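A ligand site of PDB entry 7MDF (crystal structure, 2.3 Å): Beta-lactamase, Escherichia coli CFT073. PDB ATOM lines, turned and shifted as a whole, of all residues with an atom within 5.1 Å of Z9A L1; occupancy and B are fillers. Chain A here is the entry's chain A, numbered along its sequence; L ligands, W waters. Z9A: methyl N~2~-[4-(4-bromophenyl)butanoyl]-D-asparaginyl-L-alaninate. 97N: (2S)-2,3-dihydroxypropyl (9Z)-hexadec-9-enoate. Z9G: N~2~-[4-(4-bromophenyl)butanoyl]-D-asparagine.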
ATOM      1  N   GLN A 300     -15.725   0.576  32.824  1.00  0.00           N
ATOM      2  CA  GLN A 300     -15.935  -0.569  31.939  1.00  0.00           C
ATOM      3  C   GLN A 300     -16.451  -1.759  32.745  1.00  0.00           C
ATOM      4  O   GLN A 300     -15.696  -2.376  33.499  1.00  0.00           O
ATOM      5  CB  GLN A 300     -14.649  -0.922  31.213  1.00  0.00           C
ATOM      6  CG  GLN A 300     -14.791  -2.113  30.314  1.00  0.00           C
ATOM      7  CD  GLN A 300     -13.499  -2.546  29.659  1.00  0.00           C
ATOM      8  OE1 GLN A 300     -13.485  -3.498  28.877  1.00  0.00           O
ATOM      9  NE2 GLN A 300     -12.396  -1.847  29.965  1.00  0.00           N
ATOM     10  N   ASN A 325     -20.887  -2.404  26.936  1.00  0.00           N
ATOM     11  CA  ASN A 325     -19.448  -2.158  27.085  1.00  0.00           C
ATOM     12  C   ASN A 325     -18.850  -1.817  25.706  1.00  0.00           C
ATOM     13  O   ASN A 325     -18.802  -2.680  24.823  1.00  0.00           O
ATOM     14  CB  ASN A 325     -18.761  -3.362  27.706  1.00  0.00           C
ATOM     15  CG  ASN A 325     -17.278  -3.120  27.920  1.00  0.00           C
ATOM     16  OD1 ASN A 325     -16.825  -1.977  27.898  1.00  0.00           O
ATOM     17  ND2 ASN A 325     -16.505  -4.185  28.118  1.00  0.00           N
ATOM     18  N   ASN A 327     -15.466   0.423  23.786  1.00  0.00           N
ATOM     19  CA  ASN A 327     -14.318   1.319  23.765  1.00  0.00           C
ATOM     20  C   ASN A 327     -14.662   2.675  23.142  1.00  0.00           C
ATOM     21  O   ASN A 327     -14.070   3.691  23.510  1.00  0.00           O
ATOM     22  CB  ASN A 327     -13.166   0.665  23.000  1.00  0.00           C
ATOM     23  CG  ASN A 327     -11.827   1.383  23.187  1.00  0.00           C
ATOM     24  OD1 ASN A 327     -11.501   1.853  24.288  1.00  0.00           O
ATOM     25  ND2 ASN A 327     -11.050   1.491  22.110  1.00  0.00           N
ATOM     26  N   LEU A 330     -15.746   4.519  26.026  1.00  0.00           N
ATOM     27  CA  LEU A 330     -14.609   4.808  26.895  1.00  0.00           C
ATOM     28  C   LEU A 330     -13.778   5.982  26.372  1.00  0.00           C
ATOM     29  O   LEU A 330     -13.263   6.769  27.165  1.00  0.00           O
ATOM     30  CB  LEU A 330     -13.740   3.560  27.079  1.00  0.00           C
ATOM     31  CG  LEU A 330     -14.352   2.325  27.770  1.00  0.00           C
ATOM     32  CD1 LEU A 330     -13.362   1.145  27.809  1.00  0.00           C
ATOM     33  CD2 LEU A 330     -14.829   2.654  29.166  1.00  0.00           C
ATOM     34  N   GLN A 331     -13.683   6.137  25.035  1.00  0.00           N
ATOM     35  CA  GLN A 331     -12.888   7.205  24.440  1.00  0.00           C
ATOM     36  C   GLN A 331     -13.680   8.468  24.136  1.00  0.00           C
ATOM     37  O   GLN A 331     -13.062   9.491  23.838  1.00  0.00           O
ATOM     38  CB  GLN A 331     -12.227   6.718  23.144  1.00  0.00           C
ATOM     39  CG  GLN A 331     -11.440   5.417  23.319  1.00  0.00           C
ATOM     40  CD  GLN A 331     -10.446   5.477  24.486  1.00  0.00           C
ATOM     41  OE1 GLN A 331      -9.745   6.472  24.665  1.00  0.00           O
ATOM     42  NE2 GLN A 331     -10.416   4.411  25.278  1.00  0.00           N
ATOM     43  N   GLY A 350     -10.610   1.376  17.876  1.00  0.00           N
ATOM     44  CA  GLY A 350     -11.087   0.007  17.749  1.00  0.00           C
ATOM     45  C   GLY A 350     -11.770  -0.461  19.018  1.00  0.00           C
ATOM     46  O   GLY A 350     -11.786   0.229  20.043  1.00  0.00           O
ATOM     47  N   ASP A 351     -12.330  -1.667  18.965  1.00  0.00           N
ATOM     48  CA  ASP A 351     -13.080  -2.224  20.086  1.00  0.00           C
ATOM     49  C   ASP A 351     -12.805  -3.718  20.181  1.00  0.00           C
ATOM     50  O   ASP A 351     -13.076  -4.452  19.220  1.00  0.00           O
ATOM     51  CB  ASP A 351     -14.583  -1.932  19.949  1.00  0.00           C
ATOM     52  CG  ASP A 351     -15.384  -2.405  21.141  1.00  0.00           C
ATOM     53  OD1 ASP A 351     -15.195  -1.847  22.253  1.00  0.00           O
ATOM     54  OD2 ASP A 351     -16.218  -3.327  20.957  1.00  0.00           O
ATOM     55  N   ALA A 352     -12.316  -4.170  21.347  1.00  0.00           N
ATOM     56  CA  ALA A 352     -11.864  -5.556  21.500  1.00  0.00           C
ATOM     57  C   ALA A 352     -13.021  -6.540  21.383  1.00  0.00           C
ATOM     58  O   ALA A 352     -12.880  -7.582  20.733  1.00  0.00           O
ATOM     59  CB  ALA A 352     -11.153  -5.736  22.840  1.00  0.00           C
ATOM     60  N   ILE A 353     -14.159  -6.230  22.001  1.00  0.00           N
ATOM     61  CA  ILE A 353     -15.328  -7.106  21.915  1.00  0.00           C
ATOM     62  C   ILE A 353     -15.766  -7.288  20.454  1.00  0.00           C
ATOM     63  O   ILE A 353     -16.092  -8.393  20.021  1.00  0.00           O
ATOM     64  CB  ILE A 353     -16.471  -6.574  22.793  1.00  0.00           C
ATOM     65  CG1 ILE A 353     -16.047  -6.560  24.261  1.00  0.00           C
ATOM     66  CG2 ILE A 353     -17.736  -7.398  22.601  1.00  0.00           C
ATOM     67  CD1 ILE A 353     -17.121  -6.021  25.175  1.00  0.00           C
ATOM     68  N   ALA A 355     -13.901  -6.859  17.603  1.00  0.00           N
ATOM     69  CA  ALA A 355     -12.904  -7.620  16.841  1.00  0.00           C
ATOM     70  C   ALA A 355     -12.982  -9.105  17.184  1.00  0.00           C
ATOM     71  O   ALA A 355     -12.914  -9.966  16.291  1.00  0.00           O
ATOM     72  CB  ALA A 355     -11.511  -7.066  17.123  1.00  0.00           C
ATOM     73  N   THR A 356     -13.127  -9.420  18.471  1.00  0.00           N
ATOM     74  CA  THR A 356     -13.249 -10.798  18.927  1.00  0.00           C
ATOM     75  C   THR A 356     -14.540 -11.446  18.421  1.00  0.00           C
ATOM     76  O   THR A 356     -14.540 -12.582  17.930  1.00  0.00           O
ATOM     77  CB  THR A 356     -13.176 -10.807  20.453  1.00  0.00           C
ATOM     78  OG1 THR A 356     -11.853 -10.432  20.869  1.00  0.00           O
ATOM     79  CG2 THR A 356     -13.482 -12.147  21.012  1.00  0.00           C
ATOM     80  N   PHE A 360     -14.868 -14.641  15.845  1.00  0.00           N
ATOM     81  CA  PHE A 360     -15.581 -15.855  16.193  1.00  0.00           C
ATOM     82  C   PHE A 360     -16.694 -16.184  15.191  1.00  0.00           C
ATOM     83  O   PHE A 360     -16.982 -17.371  14.967  1.00  0.00           O
ATOM     84  CB  PHE A 360     -16.146 -15.749  17.606  1.00  0.00           C
ATOM     85  CG  PHE A 360     -15.083 -15.669  18.649  1.00  0.00           C
ATOM     86  CD1 PHE A 360     -13.792 -16.063  18.354  1.00  0.00           C
ATOM     87  CD2 PHE A 360     -15.371 -15.224  19.922  1.00  0.00           C
ATOM     88  CE1 PHE A 360     -12.799 -15.997  19.302  1.00  0.00           C
ATOM     89  CE2 PHE A 360     -14.384 -15.161  20.878  1.00  0.00           C
ATOM     90  CZ  PHE A 360     -13.102 -15.546  20.565  1.00  0.00           C
ATOM     91  N   ILE A 433     -14.352 -15.676  31.392  1.00  0.00           N
ATOM     92  CA  ILE A 433     -14.337 -15.404  29.948  1.00  0.00           C
ATOM     93  C   ILE A 433     -15.754 -15.137  29.448  1.00  0.00           C
ATOM     94  O   ILE A 433     -15.989 -14.201  28.676  1.00  0.00           O
ATOM     95  CB  ILE A 433     -13.696 -16.573  29.189  1.00  0.00           C
ATOM     96  CG1 ILE A 433     -12.218 -16.721  29.566  1.00  0.00           C
ATOM     97  CG2 ILE A 433     -13.835 -16.380  27.690  1.00  0.00           C
ATOM     98  CD1 ILE A 433     -11.594 -17.951  28.961  1.00  0.00           C
ATOM     99  N   TRP A 436     -17.181 -11.604  30.305  1.00  0.00           N
ATOM    100  CA  TRP A 436     -16.635 -10.408  29.664  1.00  0.00           C
ATOM    101  C   TRP A 436     -16.604 -10.457  28.139  1.00  0.00           C
ATOM    102  O   TRP A 436     -16.714  -9.403  27.507  1.00  0.00           O
ATOM    103  CB  TRP A 436     -15.214 -10.151  30.162  1.00  0.00           C
ATOM    104  CG  TRP A 436     -15.170  -9.561  31.519  1.00  0.00           C
ATOM    105  CD1 TRP A 436     -14.962 -10.212  32.680  1.00  0.00           C
ATOM    106  CD2 TRP A 436     -15.351  -8.182  31.849  1.00  0.00           C
ATOM    107  NE1 TRP A 436     -14.993  -9.334  33.736  1.00  0.00           N
ATOM    108  CE2 TRP A 436     -15.225  -8.076  33.243  1.00  0.00           C
ATOM    109  CE3 TRP A 436     -15.579  -7.024  31.099  1.00  0.00           C
ATOM    110  CZ2 TRP A 436     -15.340  -6.858  33.914  1.00  0.00           C
ATOM    111  CZ3 TRP A 436     -15.689  -5.812  31.758  1.00  0.00           C
ATOM    112  CH2 TRP A 436     -15.565  -5.739  33.152  1.00  0.00           C
ATOM    113  N   GLY A 437     -16.443 -11.630  27.525  1.00  0.00           N
ATOM    114  CA  GLY A 437     -16.315 -11.714  26.098  1.00  0.00           C
ATOM    115  C   GLY A 437     -17.657 -11.690  25.391  1.00  0.00           C
ATOM    116  O   GLY A 437     -18.719 -11.739  26.020  1.00  0.00           O
ATOM    117  N   PRO A 438     -17.615 -11.611  24.062  1.00  0.00           N
ATOM    118  CA  PRO A 438     -18.867 -11.584  23.283  1.00  0.00           C
ATOM    119  C   PRO A 438     -19.680 -12.856  23.495  1.00  0.00           C
ATOM    120  O   PRO A 438     -19.167 -13.889  23.919  1.00  0.00           O
ATOM    121  CB  PRO A 438     -18.384 -11.481  21.823  1.00  0.00           C
ATOM    122  CG  PRO A 438     -16.936 -11.208  21.866  1.00  0.00           C
ATOM    123  CD  PRO A 438     -16.406 -11.591  23.204  1.00  0.00           C
ATOM    124  N   VAL A 441     -18.431 -16.354  21.985  1.00  0.00           N
ATOM    125  CA  VAL A 441     -17.308 -17.167  22.460  1.00  0.00           C
ATOM    126  C   VAL A 441     -17.719 -18.619  22.649  1.00  0.00           C
ATOM    127  O   VAL A 441     -16.919 -19.539  22.401  1.00  0.00           O
ATOM    128  CB  VAL A 441     -16.714 -16.593  23.766  1.00  0.00           C
ATOM    129  CG1 VAL A 441     -16.282 -15.161  23.588  1.00  0.00           C
ATOM    130  CG2 VAL A 441     -17.697 -16.709  24.908  1.00  0.00           C
HETATM  131  C18 Z9A L   1     -12.532  -5.750  26.937  1.00  0.00           C
HETATM  132  C19 Z9A L   1     -12.309  -7.089  26.259  1.00  0.00           C
HETATM  133  C20 Z9A L   1     -13.155  -8.107  26.995  1.00  0.00           C
HETATM  134  C21 Z9A L   1     -13.070  -9.491  26.373  1.00  0.00           C
HETATM  135  C22 Z9A L   1     -12.843 -10.586  27.201  1.00  0.00           C
HETATM  136  C15 Z9A L   1      -9.197  -3.829  19.102  1.00  0.00           C
HETATM  137  C11 Z9A L   1      -9.189  -1.504  22.075  1.00  0.00           C
HETATM  138  C12 Z9A L   1      -8.119  -0.436  21.830  1.00  0.00           C
HETATM  139  C13 Z9A L   1      -8.960  -2.705  21.179  1.00  0.00           C
HETATM  140  C02 Z9A L   1     -11.437  -4.746  26.635  1.00  0.00           C
HETATM  141  C04 Z9A L   1     -10.616  -2.683  25.545  1.00  0.00           C
HETATM  142  C05 Z9A L   1     -10.997  -1.459  26.359  1.00  0.00           C
HETATM  143  C06 Z9A L   1      -9.878  -0.546  26.817  1.00  0.00           C
HETATM  144  C09 Z9A L   1     -10.509  -2.259  24.087  1.00  0.00           C
HETATM  145  C23 Z9A L   1     -12.779 -11.854  26.645  1.00  0.00           C
HETATM  146  C24 Z9A L   1     -12.932 -12.013  25.276  1.00  0.00           C
HETATM  147  C26 Z9A L   1     -13.158 -10.909  24.452  1.00  0.00           C
HETATM  148  C27 Z9A L   1     -13.224  -9.634  24.994  1.00  0.00           C
HETATM  149  N03 Z9A L   1     -11.694  -3.612  25.781  1.00  0.00           N
HETATM  150  N07 Z9A L   1      -9.682   0.726  26.149  1.00  0.00           N
HETATM  151  N10 Z9A L   1      -9.215  -1.914  23.484  1.00  0.00           N
HETATM  152  O01 Z9A L   1     -10.353  -4.872  27.105  1.00  0.00           O
HETATM  153  O08 Z9A L   1      -9.194  -0.874  27.730  1.00  0.00           O
HETATM  154  O14 Z9A L   1      -9.243  -2.618  19.817  1.00  0.00           O
HETATM  155  O16 Z9A L   1      -8.547  -3.715  21.649  1.00  0.00           O
HETATM  156  O17 Z9A L   1     -11.506  -2.189  23.437  1.00  0.00           O
HETATM  157 BR25 Z9A L   1     -12.849 -13.787  24.515  1.00  0.00          BR
HETATM  158  O   97N L   2      -7.203  -7.806  26.478  1.00  0.00           O
HETATM  159  O1  97N L   2      -7.878  -5.694  26.145  1.00  0.00           O
HETATM  160  O2  97N L   2      -7.508  -4.430  28.364  1.00  0.00           O
HETATM  161  O3  97N L   2      -5.616  -2.721  28.958  1.00  0.00           O
HETATM  162  C6  97N L   2      -9.385 -14.552  20.433  1.00  0.00           C
HETATM  163  C7  97N L   2      -8.719 -14.517  21.567  1.00  0.00           C
HETATM  164  C8  97N L   2      -8.170 -13.180  22.091  1.00  0.00           C
HETATM  165  C9  97N L   2      -9.118 -12.563  23.117  1.00  0.00           C
HETATM  166  C10 97N L   2      -8.283 -11.719  24.086  1.00  0.00           C
HETATM  167  C11 97N L   2      -9.170 -11.021  25.114  1.00  0.00           C
HETATM  168  C12 97N L   2      -9.365  -9.546  24.764  1.00  0.00           C
HETATM  169  C13 97N L   2      -8.085  -8.950  24.176  1.00  0.00           C
HETATM  170  C14 97N L   2      -8.127  -7.431  24.322  1.00  0.00           C
HETATM  171  C15 97N L   2      -7.691  -7.021  25.730  1.00  0.00           C
HETATM  172  C16 97N L   2      -6.716  -4.908  26.163  1.00  0.00           C
HETATM  173  C17 97N L   2      -6.875  -3.846  27.261  1.00  0.00           C
HETATM  174  C18 97N L   2      -5.507  -3.301  27.684  1.00  0.00           C
HETATM  175  C13 Z9G L   3     -11.911  -5.790  32.399  1.00  0.00           C
HETATM  176  C14 Z9G L   3     -11.462  -5.872  30.963  1.00  0.00           C
HETATM  177  C15 Z9G L   3     -11.022  -7.273  30.547  1.00  0.00           C
HETATM  178  C16 Z9G L   3      -9.799  -7.473  29.935  1.00  0.00           C
HETATM  179  C18 Z9G L   3     -10.289  -9.808  29.799  1.00  0.00           C
HETATM  180  C02 Z9G L   3     -12.125  -3.889  34.061  1.00  0.00           C
HETATM  181  C04 Z9G L   3     -13.008  -2.606  35.981  1.00  0.00           C
HETATM  182  C05 Z9G L   3     -14.372  -2.447  36.619  1.00  0.00           C
HETATM  183  C06 Z9G L   3     -14.970  -3.736  37.163  1.00  0.00           C
HETATM  184  C09 Z9G L   3     -12.173  -1.314  35.975  1.00  0.00           C
HETATM  185  C12 Z9G L   3     -12.261  -4.334  32.611  1.00  0.00           C
HETATM  186  C17 Z9G L   3      -9.426  -8.753  29.562  1.00  0.00           C
HETATM  187  C20 Z9G L   3     -11.511  -9.599  30.415  1.00  0.00           C
HETATM  188  C21 Z9G L   3     -11.884  -8.319  30.788  1.00  0.00           C
HETATM  189  N03 Z9G L   3     -13.159  -3.036  34.619  1.00  0.00           N
HETATM  190  N07 Z9G L   3     -16.153  -4.319  36.543  1.00  0.00           N
HETATM  191  O01 Z9G L   3     -11.185  -4.231  34.710  1.00  0.00           O
HETATM  192  O08 Z9G L   3     -14.475  -4.285  38.091  1.00  0.00           O
HETATM  193  O10 Z9G L   3     -11.862  -0.756  34.886  1.00  0.00           O
HETATM  194  O11 Z9G L   3     -11.764  -0.833  37.057  1.00  0.00           O
HETATM  195 BR19 Z9G L   3      -9.818 -11.595  29.276  1.00  0.00          BR
HETATM  196  O   HOH W   1     -14.164  -2.301  25.841  1.00  0.00           O
HETATM  197  O   HOH W   2      -8.275   2.672  22.458  1.00  0.00           O
HETATM  198  O   HOH W   3     -14.339  -3.872  23.702  1.00  0.00           O
HETATM  199  O   HOH W   4      -9.376  -2.971  29.296  1.00  0.00           O
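A nitrogen (N07) of Z9A L1 is in hydrogen-bond range of the side-chain amide oxygen (OD1) of Asn 327 (2.8 Å).
The backbone NH of Ala 352 sits at hydrogen-bond distance from an oxygen (O17) of Z9A L1.
N of Asp 351 lies within hydrogen-bond range of O14 of Z9A L1, 3.3 Å away.
O of Gln 300 is in hydrogen-bond range of N03 of Z9G L3 (2.9 Å).
An oxygen (O2) of 97N L2 lies within hydrogen-bond range of an oxygen (O01) of Z9A L1 (3.1 Å).
The backbone NH (N) of Asn 327 lies within hydrogen-bond range of the side-chain carboxylate (OD1) of Asp 351.
The backbone carbonyl oxygen of Gly 350 sits at hydrogen-bond distance from the side-chain amide nitrogen of Asn 327, 2.5 Å away.
The side-chain amide oxygen of Asn 327 is in hydrogen-bond range of the side-chain amide nitrogen of Gln 331, 2.9 Å away.
The backbone carbonyl oxygen of Ala 352 lies within hydrogen-bond range of the side-chain hydroxyl of Thr 356 (3.0 Å).
ND2 of Asn 325 sits at hydrogen-bond distance from OE1 of Gln 300, 3.2 Å away.
OE1 of Gln 300 touches C18 of Z9A L1, at 3.1 Å.
Leu 330 touches Z9A L1.
Gln 331 touches Z9A L1.
C of Gly 350 touches O14 of Z9A L1 (3.4 Å).
CG2 of Thr 356 touches C26 of Z9A L1 (3.7 Å).
Trp 436 touches Z9A L1.
CA of Gly 437 touches C24 of Z9A L1, 3.5 Å away.
CD of Pro 438 touches C26 of Z9A L1, at 3.5 Å.
Val 441 touches Z9A L1 (CG1 to BR25, 3.8 Å).
Hydrophobic or aromatic side chains within 4 Å of Z9A L1: Leu 330, Ala 352, Trp 436, Pro 438 and Val 441.
Along chain A the residues within 4 Å of Z9A L1 span positions 300 to 441.
Water W4 lies within hydrogen-bond range of O2 of 97N L2 (2.5 Å), O08 of Z9A L1 (2.6 Å) and NE2 of Gln 300 (3.3 Å).
Water W1 lies within hydrogen-bond range of a nitrogen (N03) of Z9A L1 (2.8 Å), the side-chain amide oxygen (OE1) of Gln 300 (3.3 Å) and the side-chain amide oxygen (OD1) of Asn 325 (3.4 Å).
Water W3 lies within hydrogen-bond range of OD1 of Asp 351, N of Ile 353, N of Ala 352 and O17 of Z9A L1.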
